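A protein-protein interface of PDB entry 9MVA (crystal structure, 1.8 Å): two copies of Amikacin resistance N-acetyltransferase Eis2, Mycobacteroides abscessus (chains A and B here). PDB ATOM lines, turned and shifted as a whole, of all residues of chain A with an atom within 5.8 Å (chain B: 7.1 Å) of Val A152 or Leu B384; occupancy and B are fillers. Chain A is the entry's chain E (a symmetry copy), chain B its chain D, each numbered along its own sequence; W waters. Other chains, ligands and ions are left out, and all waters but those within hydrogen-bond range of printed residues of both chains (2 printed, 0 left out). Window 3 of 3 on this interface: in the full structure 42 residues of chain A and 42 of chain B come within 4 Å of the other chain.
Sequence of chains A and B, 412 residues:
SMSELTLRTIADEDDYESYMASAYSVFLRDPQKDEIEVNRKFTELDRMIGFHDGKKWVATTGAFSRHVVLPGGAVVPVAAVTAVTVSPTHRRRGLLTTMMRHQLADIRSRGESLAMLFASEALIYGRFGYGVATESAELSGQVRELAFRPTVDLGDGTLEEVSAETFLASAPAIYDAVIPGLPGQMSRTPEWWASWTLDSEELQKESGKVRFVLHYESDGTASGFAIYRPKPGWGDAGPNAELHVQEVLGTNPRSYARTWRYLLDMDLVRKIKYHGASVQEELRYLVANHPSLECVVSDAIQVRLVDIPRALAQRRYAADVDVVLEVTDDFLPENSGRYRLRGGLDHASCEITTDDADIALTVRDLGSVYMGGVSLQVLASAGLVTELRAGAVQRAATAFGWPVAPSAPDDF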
ATOM      1  N   PHE A 148      -7.763   7.525 -36.195  1.00  0.00           N
ATOM      2  CA  PHE A 148      -7.428   8.329 -35.023  1.00  0.00           C
ATOM      3  C   PHE A 148      -6.013   8.887 -35.123  1.00  0.00           C
ATOM      4  O   PHE A 148      -5.166   8.380 -35.866  1.00  0.00           O
ATOM      5  CB  PHE A 148      -7.539   7.509 -33.736  1.00  0.00           C
ATOM      6  CG  PHE A 148      -8.955   7.147 -33.357  1.00  0.00           C
ATOM      7  CD1 PHE A 148     -10.042   7.786 -33.955  1.00  0.00           C
ATOM      8  CD2 PHE A 148      -9.192   6.162 -32.418  1.00  0.00           C
ATOM      9  CE1 PHE A 148     -11.334   7.446 -33.623  1.00  0.00           C
ATOM     10  CE2 PHE A 148     -10.500   5.823 -32.065  1.00  0.00           C
ATOM     11  CZ  PHE A 148     -11.570   6.470 -32.672  1.00  0.00           C
ATOM     12  N   ARG A 149      -5.758   9.935 -34.342  1.00  0.00           N
ATOM     13  CA  ARG A 149      -4.395  10.426 -34.191  1.00  0.00           C
ATOM     14  C   ARG A 149      -3.500   9.290 -33.700  1.00  0.00           C
ATOM     15  O   ARG A 149      -3.961   8.376 -33.010  1.00  0.00           O
ATOM     16  CB  ARG A 149      -4.342  11.594 -33.204  1.00  0.00           C
ATOM     17  CG  ARG A 149      -4.929  12.885 -33.739  1.00  0.00           C
ATOM     18  CD  ARG A 149      -5.093  13.911 -32.618  1.00  0.00           C
ATOM     19  NE  ARG A 149      -3.872  14.161 -31.857  1.00  0.00           N
ATOM     20  CZ  ARG A 149      -3.769  15.109 -30.931  1.00  0.00           C
ATOM     21  NH1 ARG A 149      -4.766  15.949 -30.689  1.00  0.00           N
ATOM     22  NH2 ARG A 149      -2.647  15.208 -30.219  1.00  0.00           N
ATOM     23  N   PRO A 150      -2.214   9.316 -34.046  1.00  0.00           N
ATOM     24  CA  PRO A 150      -1.347   8.173 -33.704  1.00  0.00           C
ATOM     25  C   PRO A 150      -1.117   7.971 -32.211  1.00  0.00           C
ATOM     26  O   PRO A 150      -0.736   6.861 -31.816  1.00  0.00           O
ATOM     27  CB  PRO A 150      -0.035   8.496 -34.436  1.00  0.00           C
ATOM     28  CG  PRO A 150      -0.062   9.961 -34.674  1.00  0.00           C
ATOM     29  CD  PRO A 150      -1.524  10.294 -34.906  1.00  0.00           C
ATOM     30  N   THR A 151      -1.320   8.981 -31.366  1.00  0.00           N
ATOM     31  CA  THR A 151      -1.110   8.814 -29.931  1.00  0.00           C
ATOM     32  C   THR A 151      -2.343   8.312 -29.197  1.00  0.00           C
ATOM     33  O   THR A 151      -2.303   8.177 -27.968  1.00  0.00           O
ATOM     34  CB  THR A 151      -0.647  10.126 -29.287  1.00  0.00           C
ATOM     35  OG1 THR A 151      -1.656  11.133 -29.448  1.00  0.00           O
ATOM     36  CG2 THR A 151       0.663  10.593 -29.905  1.00  0.00           C
ATOM     37  N   VAL A 152      -3.439   8.051 -29.903  1.00  0.00           N
ATOM     38  CA  VAL A 152      -4.672   7.616 -29.251  1.00  0.00           C
ATOM     39  C   VAL A 152      -4.503   6.161 -28.819  1.00  0.00           C
ATOM     40  O   VAL A 152      -4.392   5.256 -29.653  1.00  0.00           O
ATOM     41  CB  VAL A 152      -5.886   7.792 -30.167  1.00  0.00           C
ATOM     42  CG1 VAL A 152      -7.123   7.218 -29.508  1.00  0.00           C
ATOM     43  CG2 VAL A 152      -6.086   9.272 -30.476  1.00  0.00           C
ATOM     44  N   ASP A 153      -4.503   5.936 -27.511  1.00  0.00           N
ATOM     45  CA  ASP A 153      -4.248   4.623 -26.931  1.00  0.00           C
ATOM     46  C   ASP A 153      -5.561   3.852 -26.875  1.00  0.00           C
ATOM     47  O   ASP A 153      -6.528   4.325 -26.274  1.00  0.00           O
ATOM     48  CB  ASP A 153      -3.645   4.803 -25.538  1.00  0.00           C
ATOM     49  CG  ASP A 153      -3.238   3.497 -24.885  1.00  0.00           C
ATOM     50  OD1 ASP A 153      -3.378   2.424 -25.501  1.00  0.00           O
ATOM     51  OD2 ASP A 153      -2.781   3.560 -23.726  1.00  0.00           O
ATOM     52  N   LEU A 154      -5.607   2.682 -27.528  1.00  0.00           N
ATOM     53  CA  LEU A 154      -6.794   1.835 -27.484  1.00  0.00           C
ATOM     54  C   LEU A 154      -6.800   0.877 -26.301  1.00  0.00           C
ATOM     55  O   LEU A 154      -7.810   0.191 -26.084  1.00  0.00           O
ATOM     56  CB  LEU A 154      -6.940   1.028 -28.778  1.00  0.00           C
ATOM     57  CG  LEU A 154      -6.982   1.829 -30.079  1.00  0.00           C
ATOM     58  CD1 LEU A 154      -7.154   0.859 -31.239  1.00  0.00           C
ATOM     59  CD2 LEU A 154      -8.110   2.880 -30.052  1.00  0.00           C
ATOM     60  N   ALA A 257     -12.194   5.008 -26.711  1.00  0.00           N
ATOM     61  CA  ALA A 257     -11.574   4.964 -28.038  1.00  0.00           C
ATOM     62  C   ALA A 257     -11.669   3.577 -28.673  1.00  0.00           C
ATOM     63  O   ALA A 257     -11.916   3.451 -29.880  1.00  0.00           O
ATOM     64  CB  ALA A 257     -10.109   5.408 -27.948  1.00  0.00           C
ATOM     65  N   TYR A 285     -12.219  14.997 -31.358  1.00  0.00           N
ATOM     66  CA  TYR A 285     -10.808  15.327 -31.209  1.00  0.00           C
ATOM     67  C   TYR A 285      -9.902  14.118 -31.361  1.00  0.00           C
ATOM     68  O   TYR A 285      -8.695  14.287 -31.574  1.00  0.00           O
ATOM     69  CB  TYR A 285     -10.573  16.016 -29.849  1.00  0.00           C
ATOM     70  CG  TYR A 285     -11.557  17.148 -29.688  1.00  0.00           C
ATOM     71  CD1 TYR A 285     -11.368  18.348 -30.369  1.00  0.00           C
ATOM     72  CD2 TYR A 285     -12.722  16.984 -28.947  1.00  0.00           C
ATOM     73  CE1 TYR A 285     -12.285  19.378 -30.278  1.00  0.00           C
ATOM     74  CE2 TYR A 285     -13.650  18.011 -28.843  1.00  0.00           C
ATOM     75  CZ  TYR A 285     -13.428  19.203 -29.519  1.00  0.00           C
ATOM     76  OH  TYR A 285     -14.348  20.229 -29.426  1.00  0.00           O
ATOM     77  N   LEU A 286     -10.457  12.907 -31.303  1.00  0.00           N
ATOM     78  CA  LEU A 286      -9.632  11.723 -31.523  1.00  0.00           C
ATOM     79  C   LEU A 286      -9.216  11.581 -32.978  1.00  0.00           C
ATOM     80  O   LEU A 286      -8.131  11.052 -33.259  1.00  0.00           O
ATOM     81  CB  LEU A 286     -10.380  10.459 -31.092  1.00  0.00           C
ATOM     82  CG  LEU A 286     -10.740  10.366 -29.610  1.00  0.00           C
ATOM     83  CD1 LEU A 286     -11.543   9.098 -29.387  1.00  0.00           C
ATOM     84  CD2 LEU A 286      -9.460  10.379 -28.745  1.00  0.00           C
ATOM     85  N   ALA B 360       0.523  17.189 -18.553  1.00  0.00           N
ATOM     86  CA  ALA B 360       1.445  16.874 -19.637  1.00  0.00           C
ATOM     87  C   ALA B 360       0.677  16.901 -20.955  1.00  0.00           C
ATOM     88  O   ALA B 360      -0.406  16.313 -21.058  1.00  0.00           O
ATOM     89  CB  ALA B 360       2.120  15.514 -19.412  1.00  0.00           C
ATOM     90  N   LEU B 361       1.215  17.616 -21.942  1.00  0.00           N
ATOM     91  CA  LEU B 361       0.536  17.750 -23.225  1.00  0.00           C
ATOM     92  C   LEU B 361       1.553  18.057 -24.312  1.00  0.00           C
ATOM     93  O   LEU B 361       2.680  18.486 -24.039  1.00  0.00           O
ATOM     94  CB  LEU B 361      -0.560  18.836 -23.167  1.00  0.00           C
ATOM     95  CG  LEU B 361      -0.203  20.337 -23.135  1.00  0.00           C
ATOM     96  CD1 LEU B 361      -1.480  21.195 -23.202  1.00  0.00           C
ATOM     97  CD2 LEU B 361       0.627  20.726 -21.904  1.00  0.00           C
ATOM     98  N   THR B 362       1.149  17.808 -25.560  1.00  0.00           N
ATOM     99  CA  THR B 362       1.990  18.132 -26.702  1.00  0.00           C
ATOM    100  C   THR B 362       1.801  19.596 -27.078  1.00  0.00           C
ATOM    101  O   THR B 362       0.823  20.239 -26.685  1.00  0.00           O
ATOM    102  CB  THR B 362       1.632  17.255 -27.900  1.00  0.00           C
ATOM    103  OG1 THR B 362       0.266  17.514 -28.244  1.00  0.00           O
ATOM    104  CG2 THR B 362       1.789  15.792 -27.543  1.00  0.00           C
ATOM    105  N   ASP B 365      -1.549  20.211 -28.980  1.00  0.00           N
ATOM    106  CA  ASP B 365      -2.741  20.350 -28.152  1.00  0.00           C
ATOM    107  C   ASP B 365      -2.724  21.632 -27.320  1.00  0.00           C
ATOM    108  O   ASP B 365      -3.792  22.201 -27.044  1.00  0.00           O
ATOM    109  CB  ASP B 365      -2.894  19.111 -27.279  1.00  0.00           C
ATOM    110  CG  ASP B 365      -3.370  17.914 -28.081  1.00  0.00           C
ATOM    111  OD1 ASP B 365      -4.283  18.093 -28.925  1.00  0.00           O
ATOM    112  OD2 ASP B 365      -2.830  16.812 -27.890  1.00  0.00           O
ATOM    113  N   VAL B 378     -11.871  18.543 -22.160  1.00  0.00           N
ATOM    114  CA  VAL B 378     -12.320  17.526 -23.101  1.00  0.00           C
ATOM    115  C   VAL B 378     -11.121  16.772 -23.659  1.00  0.00           C
ATOM    116  O   VAL B 378     -11.151  15.542 -23.799  1.00  0.00           O
ATOM    117  CB  VAL B 378     -13.185  18.161 -24.208  1.00  0.00           C
ATOM    118  CG1 VAL B 378     -13.646  17.083 -25.202  1.00  0.00           C
ATOM    119  CG2 VAL B 378     -14.392  18.853 -23.585  1.00  0.00           C
ATOM    120  N   LEU B 379     -10.031  17.481 -23.957  1.00  0.00           N
ATOM    121  CA  LEU B 379      -8.858  16.775 -24.470  1.00  0.00           C
ATOM    122  C   LEU B 379      -8.304  15.798 -23.441  1.00  0.00           C
ATOM    123  O   LEU B 379      -7.792  14.731 -23.806  1.00  0.00           O
ATOM    124  CB  LEU B 379      -7.786  17.775 -24.908  1.00  0.00           C
ATOM    125  CG  LEU B 379      -8.150  18.690 -26.087  1.00  0.00           C
ATOM    126  CD1 LEU B 379      -6.921  19.493 -26.520  1.00  0.00           C
ATOM    127  CD2 LEU B 379      -8.703  17.888 -27.295  1.00  0.00           C
ATOM    128  N   ALA B 380      -8.405  16.129 -22.152  1.00  0.00           N
ATOM    129  CA  ALA B 380      -7.959  15.194 -21.120  1.00  0.00           C
ATOM    130  C   ALA B 380      -8.918  14.017 -21.003  1.00  0.00           C
ATOM    131  O   ALA B 380      -8.489  12.869 -20.843  1.00  0.00           O
ATOM    132  CB  ALA B 380      -7.823  15.912 -19.771  1.00  0.00           C
ATOM    133  N   SER B 381     -10.225  14.278 -21.081  1.00  0.00           N
ATOM    134  CA  SER B 381     -11.180  13.177 -21.063  1.00  0.00           C
ATOM    135  C   SER B 381     -10.980  12.265 -22.269  1.00  0.00           C
ATOM    136  O   SER B 381     -11.166  11.045 -22.168  1.00  0.00           O
ATOM    137  CB  SER B 381     -12.614  13.738 -21.010  1.00  0.00           C
ATOM    138  OG  SER B 381     -13.570  12.706 -21.089  1.00  0.00           O
ATOM    139  N   ALA B 382     -10.584  12.838 -23.410  1.00  0.00           N
ATOM    140  CA  ALA B 382     -10.288  12.065 -24.606  1.00  0.00           C
ATOM    141  C   ALA B 382      -9.002  11.261 -24.483  1.00  0.00           C
ATOM    142  O   ALA B 382      -8.760  10.385 -25.322  1.00  0.00           O
ATOM    143  CB  ALA B 382     -10.189  12.996 -25.818  1.00  0.00           C
ATOM    144  N   GLY B 383      -8.164  11.550 -23.484  1.00  0.00           N
ATOM    145  CA  GLY B 383      -6.897  10.863 -23.300  1.00  0.00           C
ATOM    146  C   GLY B 383      -5.720  11.498 -24.007  1.00  0.00           C
ATOM    147  O   GLY B 383      -4.610  10.945 -23.954  1.00  0.00           O
ATOM    148  N   LEU B 384      -5.925  12.639 -24.682  1.00  0.00           N
ATOM    149  CA  LEU B 384      -4.856  13.260 -25.455  1.00  0.00           C
ATOM    150  C   LEU B 384      -3.943  14.095 -24.578  1.00  0.00           C
ATOM    151  O   LEU B 384      -2.790  14.341 -24.953  1.00  0.00           O
ATOM    152  CB  LEU B 384      -5.451  14.124 -26.575  1.00  0.00           C
ATOM    153  CG  LEU B 384      -6.252  13.346 -27.631  1.00  0.00           C
ATOM    154  CD1 LEU B 384      -7.150  14.291 -28.467  1.00  0.00           C
ATOM    155  CD2 LEU B 384      -5.313  12.550 -28.530  1.00  0.00           C
ATOM    156  N   VAL B 385      -4.436  14.502 -23.413  1.00  0.00           N
ATOM    157  CA  VAL B 385      -3.728  15.322 -22.442  1.00  0.00           C
ATOM    158  C   VAL B 385      -3.768  14.576 -21.116  1.00  0.00           C
ATOM    159  O   VAL B 385      -4.781  13.950 -20.790  1.00  0.00           O
ATOM    160  CB  VAL B 385      -4.391  16.715 -22.326  1.00  0.00           C
ATOM    161  CG1 VAL B 385      -4.036  17.397 -21.017  1.00  0.00           C
ATOM    162  CG2 VAL B 385      -3.985  17.573 -23.515  1.00  0.00           C
ATOM    163  N   THR B 386      -2.668  14.604 -20.364  1.00  0.00           N
ATOM    164  CA  THR B 386      -2.577  13.848 -19.121  1.00  0.00           C
ATOM    165  C   THR B 386      -2.577  14.780 -17.916  1.00  0.00           C
ATOM    166  O   THR B 386      -1.730  15.675 -17.820  1.00  0.00           O
ATOM    167  CB  THR B 386      -1.305  12.996 -19.070  1.00  0.00           C
ATOM    168  OG1 THR B 386      -1.270  12.102 -20.184  1.00  0.00           O
ATOM    169  CG2 THR B 386      -1.277  12.206 -17.762  1.00  0.00           C
HETATM  170  O   HOH W   1      -4.118   8.762 -25.983  1.00  0.00           O
HETATM  171  O   HOH W   2      -1.432  13.134 -27.163  1.00  0.00           O
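Of chain A, only Arg A149, Val A152 and Tyr A285 come within 4 Å of Leu B384.
Of the printed residues of chain A, Ala B382 touches Leu A286 (3.5 Å).
Of the printed residues of chain A, Leu B379 touches Tyr A285.
Of the printed residues of chain B, Tyr A285 touches Val B378, Leu B379 and Leu B384.
CD1 of Leu B384 touches NH1 of Arg A149 (3.7 Å).
CG2 of Val A152 touches CD2 of Leu B384, 3.9 Å away.
Tyr A285 touches Val B378.
CB of Tyr A285 touches CD2 of Leu B379, 3.7 Å away.
Leu B384 touches Tyr A285.
Leu A286 touches Ala B382.
The guanidinium group of Arg A149 is in salt-bridge range of the side-chain carboxylate of Asp B365 (2.8 Å).
The backbone carbonyl oxygen of Leu B379 lies within hydrogen-bond range of the backbone NH of Leu B384.
OG1 of Thr B362 is in hydrogen-bond range of OD2 of Asp B365 (3.2 Å).
N of Val B385 sits at hydrogen-bond distance from O of Leu B379 (3.4 Å).
The backbone NH (N) of Arg A149 sits at hydrogen-bond distance from the backbone carbonyl oxygen (O) of Leu A286, at 2.8 Å.
No position is printed for both chains.
Of the 7 pairs that touch across the chains among the printed residues, none has its exchanged pair printed and touching as well.
Water W1 lies within hydrogen-bond range of O of Thr A151 (2.8 Å), O of Gly B383 (3.0 Å) and N of Asp A153 (3.2 Å).
Water W2 bridges the backbone carbonyl oxygen of Leu B384 (2.9 Å) and the side-chain hydroxyl of Thr A151 (3.0 Å).
Of the 13 printed residues of chain B, 5 touch a printed residue of chain A.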
